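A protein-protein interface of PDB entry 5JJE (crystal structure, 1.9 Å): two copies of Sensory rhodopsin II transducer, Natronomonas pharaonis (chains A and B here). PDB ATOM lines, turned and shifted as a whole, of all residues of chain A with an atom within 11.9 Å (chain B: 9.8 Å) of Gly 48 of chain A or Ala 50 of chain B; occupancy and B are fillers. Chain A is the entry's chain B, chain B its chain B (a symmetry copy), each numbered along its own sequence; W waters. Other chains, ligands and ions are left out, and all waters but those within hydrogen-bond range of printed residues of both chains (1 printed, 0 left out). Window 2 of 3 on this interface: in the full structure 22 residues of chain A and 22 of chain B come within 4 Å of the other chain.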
ATOM      1  N   TYR A  38     -34.123 -18.587 -18.358  1.00  0.00           N
ATOM      2  CA  TYR A  38     -34.109 -19.583 -17.297  1.00  0.00           C
ATOM      3  C   TYR A  38     -32.877 -20.481 -17.393  1.00  0.00           C
ATOM      4  O   TYR A  38     -32.283 -20.837 -16.377  1.00  0.00           O
ATOM      5  CB  TYR A  38     -35.377 -20.440 -17.339  1.00  0.00           C
ATOM      6  CG  TYR A  38     -35.345 -21.631 -16.402  1.00  0.00           C
ATOM      7  CD1 TYR A  38     -35.458 -21.461 -15.030  1.00  0.00           C
ATOM      8  CD2 TYR A  38     -35.201 -22.924 -16.892  1.00  0.00           C
ATOM      9  CE1 TYR A  38     -35.430 -22.545 -14.167  1.00  0.00           C
ATOM     10  CE2 TYR A  38     -35.169 -24.016 -16.037  1.00  0.00           C
ATOM     11  CZ  TYR A  38     -35.287 -23.821 -14.675  1.00  0.00           C
ATOM     12  OH  TYR A  38     -35.248 -24.905 -13.815  1.00  0.00           O
ATOM     13  N   GLY A  39     -32.496 -20.850 -18.613  1.00  0.00           N
ATOM     14  CA  GLY A  39     -31.348 -21.721 -18.807  1.00  0.00           C
ATOM     15  C   GLY A  39     -30.073 -21.048 -18.342  1.00  0.00           C
ATOM     16  O   GLY A  39     -29.189 -21.675 -17.755  1.00  0.00           O
ATOM     17  N   GLU A  40     -29.991 -19.752 -18.609  1.00  0.00           N
ATOM     18  CA  GLU A  40     -28.864 -18.934 -18.187  1.00  0.00           C
ATOM     19  C   GLU A  40     -28.770 -18.848 -16.669  1.00  0.00           C
ATOM     20  O   GLU A  40     -27.677 -18.893 -16.101  1.00  0.00           O
ATOM     21  CB  GLU A  40     -29.019 -17.534 -18.763  1.00  0.00           C
ATOM     22  CG  GLU A  40     -27.766 -16.708 -18.718  1.00  0.00           C
ATOM     23  CD  GLU A  40     -27.506 -16.038 -20.044  1.00  0.00           C
ATOM     24  OE1 GLU A  40     -26.806 -16.639 -20.883  1.00  0.00           O
ATOM     25  OE2 GLU A  40     -28.004 -14.917 -20.251  1.00  0.00           O
ATOM     26  N   VAL A  41     -29.921 -18.705 -16.015  1.00  0.00           N
ATOM     27  CA  VAL A  41     -29.973 -18.657 -14.552  1.00  0.00           C
ATOM     28  C   VAL A  41     -29.618 -20.004 -13.919  1.00  0.00           C
ATOM     29  O   VAL A  41     -28.923 -20.059 -12.891  1.00  0.00           O
ATOM     30  CB  VAL A  41     -31.373 -18.191 -14.057  1.00  0.00           C
ATOM     31  CG1 VAL A  41     -31.538 -18.413 -12.557  1.00  0.00           C
ATOM     32  CG2 VAL A  41     -31.605 -16.726 -14.418  1.00  0.00           C
ATOM     33  N   THR A  42     -30.097 -21.092 -14.515  1.00  0.00           N
ATOM     34  CA  THR A  42     -29.795 -22.417 -13.974  1.00  0.00           C
ATOM     35  C   THR A  42     -28.321 -22.737 -14.171  1.00  0.00           C
ATOM     36  O   THR A  42     -27.675 -23.296 -13.285  1.00  0.00           O
ATOM     37  CB  THR A  42     -30.640 -23.526 -14.617  1.00  0.00           C
ATOM     38  OG1 THR A  42     -30.396 -23.565 -16.027  1.00  0.00           O
ATOM     39  CG2 THR A  42     -32.098 -23.270 -14.374  1.00  0.00           C
ATOM     40  N   ALA A  43     -27.797 -22.368 -15.334  1.00  0.00           N
ATOM     41  CA  ALA A  43     -26.382 -22.571 -15.628  1.00  0.00           C
ATOM     42  C   ALA A  43     -25.512 -21.810 -14.633  1.00  0.00           C
ATOM     43  O   ALA A  43     -24.519 -22.334 -14.146  1.00  0.00           O
ATOM     44  CB  ALA A  43     -26.064 -22.148 -17.055  1.00  0.00           C
ATOM     45  N   ALA A  44     -25.894 -20.573 -14.327  1.00  0.00           N
ATOM     46  CA  ALA A  44     -25.178 -19.789 -13.324  1.00  0.00           C
ATOM     47  C   ALA A  44     -25.354 -20.401 -11.940  1.00  0.00           C
ATOM     48  O   ALA A  44     -24.441 -20.356 -11.105  1.00  0.00           O
ATOM     49  CB  ALA A  44     -25.645 -18.344 -13.331  1.00  0.00           C
ATOM     50  N   ALA A  45     -26.525 -20.984 -11.702  1.00  0.00           N
ATOM     51  CA  ALA A  45     -26.814 -21.608 -10.416  1.00  0.00           C
ATOM     52  C   ALA A  45     -25.916 -22.818 -10.196  1.00  0.00           C
ATOM     53  O   ALA A  45     -25.439 -23.055  -9.085  1.00  0.00           O
ATOM     54  CB  ALA A  45     -28.271 -22.018 -10.336  1.00  0.00           C
ATOM     55  N   ALA A  46     -25.688 -23.574 -11.265  1.00  0.00           N
ATOM     56  CA  ALA A  46     -24.874 -24.782 -11.207  1.00  0.00           C
ATOM     57  C   ALA A  46     -23.452 -24.462 -10.758  1.00  0.00           C
ATOM     58  O   ALA A  46     -22.733 -25.332 -10.267  1.00  0.00           O
ATOM     59  CB  ALA A  46     -24.863 -25.468 -12.569  1.00  0.00           C
ATOM     60  N   THR A  47     -23.106 -23.208 -10.882  1.00  0.00           N
ATOM     61  CA  THR A  47     -21.816 -22.713 -10.543  1.00  0.00           C
ATOM     62  C   THR A  47     -21.601 -22.636  -9.037  1.00  0.00           C
ATOM     63  O   THR A  47     -20.551 -22.994  -8.553  1.00  0.00           O
ATOM     64  CB  THR A  47     -21.638 -21.370 -11.201  1.00  0.00           C
ATOM     65  OG1 THR A  47     -20.942 -21.536 -12.438  1.00  0.00           O
ATOM     66  CG2 THR A  47     -20.902 -20.444 -10.346  1.00  0.00           C
ATOM     67  N   GLY A  48     -22.597 -22.169  -8.308  1.00  0.00           N
ATOM     68  CA  GLY A  48     -22.530 -22.013  -6.864  1.00  0.00           C
ATOM     69  C   GLY A  48     -22.186 -20.583  -6.489  1.00  0.00           C
ATOM     70  O   GLY A  48     -22.197 -20.211  -5.316  1.00  0.00           O
ATOM     71  N   ASP A  49     -21.917 -19.793  -7.511  1.00  0.00           N
ATOM     72  CA  ASP A  49     -21.622 -18.401  -7.315  1.00  0.00           C
ATOM     73  C   ASP A  49     -22.940 -17.613  -7.306  1.00  0.00           C
ATOM     74  O   ASP A  49     -23.628 -17.576  -8.293  1.00  0.00           O
ATOM     75  CB  ASP A  49     -20.701 -17.914  -8.426  1.00  0.00           C
ATOM     76  CG  ASP A  49     -20.326 -16.497  -8.262  1.00  0.00           C
ATOM     77  OD1 ASP A  49     -20.740 -15.944  -7.263  1.00  0.00           O
ATOM     78  OD2 ASP A  49     -19.628 -15.912  -9.101  1.00  0.00           O
ATOM     79  N   ALA A  50     -23.265 -17.004  -6.175  1.00  0.00           N
ATOM     80  CA  ALA A  50     -24.483 -16.202  -6.046  1.00  0.00           C
ATOM     81  C   ALA A  50     -24.460 -14.972  -6.947  1.00  0.00           C
ATOM     82  O   ALA A  50     -25.487 -14.590  -7.531  1.00  0.00           O
ATOM     83  CB  ALA A  50     -24.683 -15.784  -4.593  1.00  0.00           C
ATOM     84  N   ALA A  51     -23.290 -14.349  -7.053  1.00  0.00           N
ATOM     85  CA  ALA A  51     -23.145 -13.132  -7.849  1.00  0.00           C
ATOM     86  C   ALA A  51     -23.345 -13.406  -9.338  1.00  0.00           C
ATOM     87  O   ALA A  51     -23.878 -12.565 -10.070  1.00  0.00           O
ATOM     88  CB  ALA A  51     -21.792 -12.487  -7.601  1.00  0.00           C
ATOM     89  N   ALA A  52     -22.916 -14.586  -9.777  1.00  0.00           N
ATOM     90  CA  ALA A  52     -23.111 -14.993 -11.162  1.00  0.00           C
ATOM     91  C   ALA A  52     -24.604 -15.109 -11.465  1.00  0.00           C
ATOM     92  O   ALA A  52     -25.053 -14.690 -12.522  1.00  0.00           O
ATOM     93  CB  ALA A  52     -22.413 -16.311 -11.442  1.00  0.00           C
ATOM     94  N   VAL A  53     -25.359 -15.688 -10.533  1.00  0.00           N
ATOM     95  CA  VAL A  53     -26.798 -15.866 -10.716  1.00  0.00           C
ATOM     96  C   VAL A  53     -27.512 -14.517 -10.775  1.00  0.00           C
ATOM     97  O   VAL A  53     -28.403 -14.315 -11.610  1.00  0.00           O
ATOM     98  CB  VAL A  53     -27.420 -16.738  -9.606  1.00  0.00           C
ATOM     99  CG1 VAL A  53     -28.878 -17.052  -9.926  1.00  0.00           C
ATOM    100  CG2 VAL A  53     -26.623 -18.026  -9.442  1.00  0.00           C
ATOM    101  N   GLN A  54     -27.111 -13.596  -9.901  1.00  0.00           N
ATOM    102  CA  GLN A  54     -27.669 -12.245  -9.900  1.00  0.00           C
ATOM    103  C   GLN A  54     -27.430 -11.594 -11.252  1.00  0.00           C
ATOM    104  O   GLN A  54     -28.305 -10.924 -11.808  1.00  0.00           O
ATOM    105  CB  GLN A  54     -27.019 -11.400  -8.804  1.00  0.00           C
ATOM    106  CG  GLN A  54     -27.400  -9.925  -8.848  1.00  0.00           C
ATOM    107  CD  GLN A  54     -26.760  -9.122  -7.727  1.00  0.00           C
ATOM    108  OE1 GLN A  54     -25.864  -9.605  -7.038  1.00  0.00           O
ATOM    109  NE2 GLN A  54     -27.219  -7.889  -7.543  1.00  0.00           N
ATOM    110  N   GLU A  55     -26.230 -11.809 -11.778  1.00  0.00           N
ATOM    111  CA  GLU A  55     -25.856 -11.276 -13.074  1.00  0.00           C
ATOM    112  C   GLU A  55     -26.756 -11.823 -14.188  1.00  0.00           C
ATOM    113  O   GLU A  55     -27.248 -11.068 -15.019  1.00  0.00           O
ATOM    114  CB  GLU A  55     -24.384 -11.586 -13.355  1.00  0.00           C
ATOM    115  CG  GLU A  55     -23.837 -10.936 -14.608  1.00  0.00           C
ATOM    116  CD  GLU A  55     -22.357 -11.208 -14.798  1.00  0.00           C
ATOM    117  OE1 GLU A  55     -21.730 -11.771 -13.872  1.00  0.00           O
ATOM    118  OE2 GLU A  55     -21.825 -10.861 -15.871  1.00  0.00           O
ATOM    119  N   ALA A  56     -26.975 -13.133 -14.197  1.00  0.00           N
ATOM    120  CA  ALA A  56     -27.830 -13.751 -15.205  1.00  0.00           C
ATOM    121  C   ALA A  56     -29.281 -13.300 -15.033  1.00  0.00           C
ATOM    122  O   ALA A  56     -30.034 -13.225 -16.001  1.00  0.00           O
ATOM    123  CB  ALA A  56     -27.752 -15.254 -15.119  1.00  0.00           C
ATOM    124  N   ALA A  57     -29.651 -13.021 -13.789  1.00  0.00           N
ATOM    125  CA  ALA A  57     -31.022 -12.683 -13.429  1.00  0.00           C
ATOM    126  C   ALA A  57     -31.328 -11.249 -13.798  1.00  0.00           C
ATOM    127  O   ALA A  57     -32.427 -10.943 -14.274  1.00  0.00           O
ATOM    128  CB  ALA A  57     -31.256 -12.907 -11.925  1.00  0.00           C
ATOM    129  N   VAL A  58     -30.359 -10.369 -13.577  1.00  0.00           N
ATOM    130  CA  VAL A  58     -30.524  -8.967 -13.941  1.00  0.00           C
ATOM    131  C   VAL A  58     -30.681  -8.850 -15.465  1.00  0.00           C
ATOM    132  O   VAL A  58     -31.519  -8.093 -15.958  1.00  0.00           O
ATOM    133  CB  VAL A  58     -29.350  -8.120 -13.412  1.00  0.00           C
ATOM    134  CG1 VAL A  58     -29.296  -6.767 -14.078  1.00  0.00           C
ATOM    135  CG2 VAL A  58     -29.472  -7.956 -11.880  1.00  0.00           C
ATOM    136  N   VAL B  41     -34.191 -10.178  -6.218  1.00  0.00           N
ATOM    137  CA  VAL B  41     -32.947 -10.827  -6.638  1.00  0.00           C
ATOM    138  C   VAL B  41     -31.730 -10.274  -5.895  1.00  0.00           C
ATOM    139  O   VAL B  41     -30.819 -11.029  -5.517  1.00  0.00           O
ATOM    140  CB  VAL B  41     -32.738 -10.693  -8.174  1.00  0.00           C
ATOM    141  CG1 VAL B  41     -31.326 -11.100  -8.583  1.00  0.00           C
ATOM    142  CG2 VAL B  41     -33.780 -11.516  -8.928  1.00  0.00           C
ATOM    143  N   ALA B  43     -31.793  -8.797  -2.942  1.00  0.00           N
ATOM    144  CA  ALA B  43     -31.959  -9.223  -1.556  1.00  0.00           C
ATOM    145  C   ALA B  43     -31.486 -10.661  -1.376  1.00  0.00           C
ATOM    146  O   ALA B  43     -30.812 -10.978  -0.404  1.00  0.00           O
ATOM    147  CB  ALA B  43     -33.410  -9.075  -1.120  1.00  0.00           C
ATOM    148  N   ALA B  44     -31.835 -11.530  -2.321  1.00  0.00           N
ATOM    149  CA  ALA B  44     -31.364 -12.912  -2.287  1.00  0.00           C
ATOM    150  C   ALA B  44     -29.859 -12.971  -2.507  1.00  0.00           C
ATOM    151  O   ALA B  44     -29.166 -13.825  -1.938  1.00  0.00           O
ATOM    152  CB  ALA B  44     -32.088 -13.756  -3.321  1.00  0.00           C
ATOM    153  N   ALA B  45     -29.350 -12.054  -3.325  1.00  0.00           N
ATOM    154  CA  ALA B  45     -27.922 -12.004  -3.613  1.00  0.00           C
ATOM    155  C   ALA B  45     -27.135 -11.644  -2.360  1.00  0.00           C
ATOM    156  O   ALA B  45     -26.059 -12.190  -2.113  1.00  0.00           O
ATOM    157  CB  ALA B  45     -27.633 -11.005  -4.716  1.00  0.00           C
ATOM    158  N   ALA B  46     -27.686 -10.725  -1.574  1.00  0.00           N
ATOM    159  CA  ALA B  46     -27.040 -10.253  -0.354  1.00  0.00           C
ATOM    160  C   ALA B  46     -26.825 -11.399   0.629  1.00  0.00           C
ATOM    161  O   ALA B  46     -25.972 -11.322   1.513  1.00  0.00           O
ATOM    162  CB  ALA B  46     -27.877  -9.151   0.285  1.00  0.00           C
ATOM    163  N   THR B  47     -27.562 -12.456   0.411  1.00  0.00           N
ATOM    164  CA  THR B  47     -27.528 -13.619   1.230  1.00  0.00           C
ATOM    165  C   THR B  47     -26.264 -14.441   1.018  1.00  0.00           C
ATOM    166  O   THR B  47     -25.676 -14.910   1.966  1.00  0.00           O
ATOM    167  CB  THR B  47     -28.770 -14.425   0.957  1.00  0.00           C
ATOM    168  OG1 THR B  47     -29.766 -14.108   1.931  1.00  0.00           O
ATOM    169  CG2 THR B  47     -28.500 -15.858   0.983  1.00  0.00           C
ATOM    170  N   GLY B  48     -25.856 -14.612  -0.226  1.00  0.00           N
ATOM    171  CA  GLY B  48     -24.684 -15.394  -0.586  1.00  0.00           C
ATOM    172  C   GLY B  48     -25.077 -16.798  -1.003  1.00  0.00           C
ATOM    173  O   GLY B  48     -24.246 -17.584  -1.459  1.00  0.00           O
ATOM    174  N   ASP B  49     -26.359 -17.077  -0.868  1.00  0.00           N
ATOM    175  CA  ASP B  49     -26.887 -18.351  -1.268  1.00  0.00           C
ATOM    176  C   ASP B  49     -27.260 -18.287  -2.756  1.00  0.00           C
ATOM    177  O   ASP B  49     -28.127 -17.540  -3.129  1.00  0.00           O
ATOM    178  CB  ASP B  49     -28.102 -18.690  -0.413  1.00  0.00           C
ATOM    179  CG  ASP B  49     -28.671 -20.009  -0.747  1.00  0.00           C
ATOM    180  OD1 ASP B  49     -28.078 -20.653  -1.590  1.00  0.00           O
ATOM    181  OD2 ASP B  49     -29.697 -20.430  -0.195  1.00  0.00           O
ATOM    182  N   ALA B  50     -26.581 -19.074  -3.578  1.00  0.00           N
ATOM    183  CA  ALA B  50     -26.858 -19.122  -5.014  1.00  0.00           C
ATOM    184  C   ALA B  50     -28.253 -19.660  -5.313  1.00  0.00           C
ATOM    185  O   ALA B  50     -28.940 -19.178  -6.229  1.00  0.00           O
ATOM    186  CB  ALA B  50     -25.806 -19.970  -5.723  1.00  0.00           C
ATOM    187  N   ALA B  51     -28.667 -20.665  -4.547  1.00  0.00           N
ATOM    188  CA  ALA B  51     -29.967 -21.300  -4.760  1.00  0.00           C
ATOM    189  C   ALA B  51     -31.117 -20.344  -4.453  1.00  0.00           C
ATOM    190  O   ALA B  51     -32.167 -20.388  -5.105  1.00  0.00           O
ATOM    191  CB  ALA B  51     -30.087 -22.566  -3.930  1.00  0.00           C
ATOM    192  N   ALA B  52     -30.913 -19.484  -3.460  1.00  0.00           N
ATOM    193  CA  ALA B  52     -31.907 -18.476  -3.115  1.00  0.00           C
ATOM    194  C   ALA B  52     -32.098 -17.512  -4.284  1.00  0.00           C
ATOM    195  O   ALA B  52     -33.218 -17.139  -4.600  1.00  0.00           O
ATOM    196  CB  ALA B  52     -31.498 -17.717  -1.866  1.00  0.00           C
ATOM    197  N   VAL B  53     -30.994 -17.109  -4.911  1.00  0.00           N
ATOM    198  CA  VAL B  53     -31.049 -16.177  -6.035  1.00  0.00           C
ATOM    199  C   VAL B  53     -31.767 -16.804  -7.229  1.00  0.00           C
ATOM    200  O   VAL B  53     -32.582 -16.145  -7.887  1.00  0.00           O
ATOM    201  CB  VAL B  53     -29.646 -15.699  -6.462  1.00  0.00           C
ATOM    202  CG1 VAL B  53     -29.752 -14.597  -7.510  1.00  0.00           C
ATOM    203  CG2 VAL B  53     -28.868 -15.205  -5.249  1.00  0.00           C
ATOM    204  N   GLN B  54     -31.474 -18.075  -7.496  1.00  0.00           N
ATOM    205  CA  GLN B  54     -32.143 -18.807  -8.570  1.00  0.00           C
ATOM    206  C   GLN B  54     -33.642 -18.823  -8.320  1.00  0.00           C
ATOM    207  O   GLN B  54     -34.448 -18.645  -9.236  1.00  0.00           O
ATOM    208  CB  GLN B  54     -31.621 -20.243  -8.641  1.00  0.00           C
ATOM    209  CG  GLN B  54     -32.392 -21.137  -9.605  1.00  0.00           C
ATOM    210  CD  GLN B  54     -31.829 -22.547  -9.673  1.00  0.00           C
ATOM    211  OE1 GLN B  54     -30.998 -22.934  -8.852  1.00  0.00           O
ATOM    212  NE2 GLN B  54     -32.280 -23.321 -10.654  1.00  0.00           N
ATOM    213  N   GLU B  55     -34.001 -19.032  -7.059  1.00  0.00           N
ATOM    214  CA  GLU B  55     -35.394 -19.051  -6.654  1.00  0.00           C
ATOM    215  C   GLU B  55     -36.076 -17.706  -6.925  1.00  0.00           C
ATOM    216  O   GLU B  55     -37.169 -17.662  -7.479  1.00  0.00           O
ATOM    217  CB  GLU B  55     -35.497 -19.431  -5.175  1.00  0.00           C
ATOM    218  CG  GLU B  55     -36.912 -19.643  -4.682  1.00  0.00           C
ATOM    219  CD  GLU B  55     -36.955 -20.096  -3.235  1.00  0.00           C
ATOM    220  OE1 GLU B  55     -35.878 -20.392  -2.670  1.00  0.00           O
ATOM    221  OE2 GLU B  55     -38.063 -20.153  -2.666  1.00  0.00           O
ATOM    222  N   ALA B  56     -35.428 -16.612  -6.540  1.00  0.00           N
ATOM    223  CA  ALA B  56     -35.984 -15.282  -6.766  1.00  0.00           C
ATOM    224  C   ALA B  56     -36.047 -14.970  -8.262  1.00  0.00           C
ATOM    225  O   ALA B  56     -36.915 -14.227  -8.713  1.00  0.00           O
ATOM    226  CB  ALA B  56     -35.160 -14.234  -6.063  1.00  0.00           C
ATOM    227  N   ALA B  57     -35.105 -15.538  -9.006  1.00  0.00           N
ATOM    228  CA  ALA B  57     -34.948 -15.264 -10.429  1.00  0.00           C
ATOM    229  C   ALA B  57     -35.981 -16.022 -11.230  1.00  0.00           C
ATOM    230  O   ALA B  57     -36.536 -15.494 -12.201  1.00  0.00           O
ATOM    231  CB  ALA B  57     -33.531 -15.636 -10.897  1.00  0.00           C
ATOM    232  N   VAL B  58     -36.239 -17.261 -10.829  1.00  0.00           N
ATOM    233  CA  VAL B  58     -37.252 -18.068 -11.496  1.00  0.00           C
ATOM    234  C   VAL B  58     -38.630 -17.411 -11.315  1.00  0.00           C
ATOM    235  O   VAL B  58     -39.427 -17.344 -12.251  1.00  0.00           O
ATOM    236  CB  VAL B  58     -37.229 -19.520 -10.977  1.00  0.00           C
ATOM    237  CG1 VAL B  58     -38.481 -20.267 -11.361  1.00  0.00           C
ATOM    238  CG2 VAL B  58     -35.982 -20.251 -11.526  1.00  0.00           C
HETATM  239  O   HOH W   1     -35.305 -24.082 -10.733  1.00  0.00           O
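Water W1 bridges the side-chain amide nitrogen (NE2) of Gln 54 of chain B and the side-chain hydroxyl (OH) of Tyr 38 of chain A.
Ala 45 of chain A touches Gln 54 of chain B, and with the chains exchanged Gln 54 of chain A touches Ala 45 of chain B.
Gly 48 of chain A touches Ala 50 of chain B, and with the chains exchanged Ala 50 of chain A touches Gly 48 of chain B.
Ala 50 of chain A touches its own counterpart, Ala 50 of chain B.
Val 53 of chain A touches its own counterpart, Val 53 of chain B.
Of the 13 pairs that touch across the chains among the printed residues, 11 have their exchanged pair printed and touching as well.
The side-chain hydroxyl of Thr 42 of chain A sits at hydrogen-bond distance from the backbone carbonyl oxygen of Gly 39 of chain A, 2.8 Å away.
The backbone carbonyl oxygen (O) of Tyr 38 of chain A lies close to the side-chain hydroxyl (OG1) of Thr 42 of chain A (3.3 Å).
Among the printed residues, pairs that only touch across the chains: Ala 45 of chain A with Gln 54 of chain B (3.2 Å), Gln 54 of chain A with Ala 45 of chain B (3.2 Å), Tyr 38 of chain A with Val 58 of chain B (3.5 Å), Val 53 of chain A with Val 53 of chain B (3.6 Å), Gly 48 of chain A with Ala 50 of chain B (3.6 Å), Ala 50 of chain A with Gly 48 of chain B (3.6 Å), Ala 57 of chain A with Ala 57 of chain B (3.7 Å), Val 53 of chain A with Gln 54 of chain B (3.7 Å), Gln 54 of chain A with Val 53 of chain B (3.7 Å), Thr 42 of chain A with Gln 54 of chain B (3.7 Å), Ala 57 of chain A with Val 41 of chain B (3.8 Å), Val 41 of chain A with Ala 57 of chain B (3.8 Å) and Ala 50 of chain A with Ala 50 of chain B (3.9 Å).
Hydrophobic or aromatic side chains of chain A that line the printed part of chain B: Tyr 38, Val 41, Ala 45, Ala 50, Val 53 and Ala 57.
Along chain A the printed residues that touch a printed residue of chain B span positions 38 to 57.
Of the 17 printed residues of chain B, 8 touch a printed residue of chain A.
Hydrophobic or aromatic side chains of chain B within 4 Å of the printed part of chain A: Val 41, Ala 45, Ala 50, Val 53, Ala 57 and Val 58.
Among the printed residues, no Asp or Glu carboxylate lies within 4 Å of a Lys or Arg side-chain nitrogen of the other chain.
Of chain A, only Gly 48 (3.6 Å) and Ala 50 (3.9 Å) come within 4 Å of Ala 50 of chain B.
Of chain B, only Gln 54 (3.2 Å) comes within 4 Å of Ala 45 of chain A.
Ala 50 of chain A touches just these residues of chain B: Gly 48 and Ala 50.
Of the printed residues of chain A, Gly 48 of chain B touches Ala 50 (3.6 Å).
No residue of chain A comes within 4 Å of Ala 51 of chain B.
No residue of chain A comes within 4 Å of Ala 52 of chain B.
Of the printed residues of chain A, Val 53 of chain B touches Val 53 (3.6 Å) and Gln 54 (3.7 Å).
Of chain A, only Thr 42, Ala 45 and Val 53 come within 4 Å of Gln 54 of chain B.
Of the printed residues of chain B, Tyr 38 of chain A touches Val 58.
Printed residues of chain B within 4 Å of Ala 57 of chain A: Val 41 and Ala 57.
Printed residues of chain B within 4 Å of Val 53 of chain A: Val 53 and Gln 54.
Of the printed residues of chain B, Thr 42 of chain A touches Gln 54.
Ala 51 of chain A touches none of the printed residues of chain B.
The nearest residue of chain B that does not touch Gly 48 of chain A is Gly 48 of chain B (5.1 Å).
The nearest residue of chain A that does not touch Ala 50 of chain B is Asp 49 of chain A (4.03 Å).
The nearest printed residue of chain B that does not touch Tyr 38 of chain A is Gln 54 of chain B (4.6 Å).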
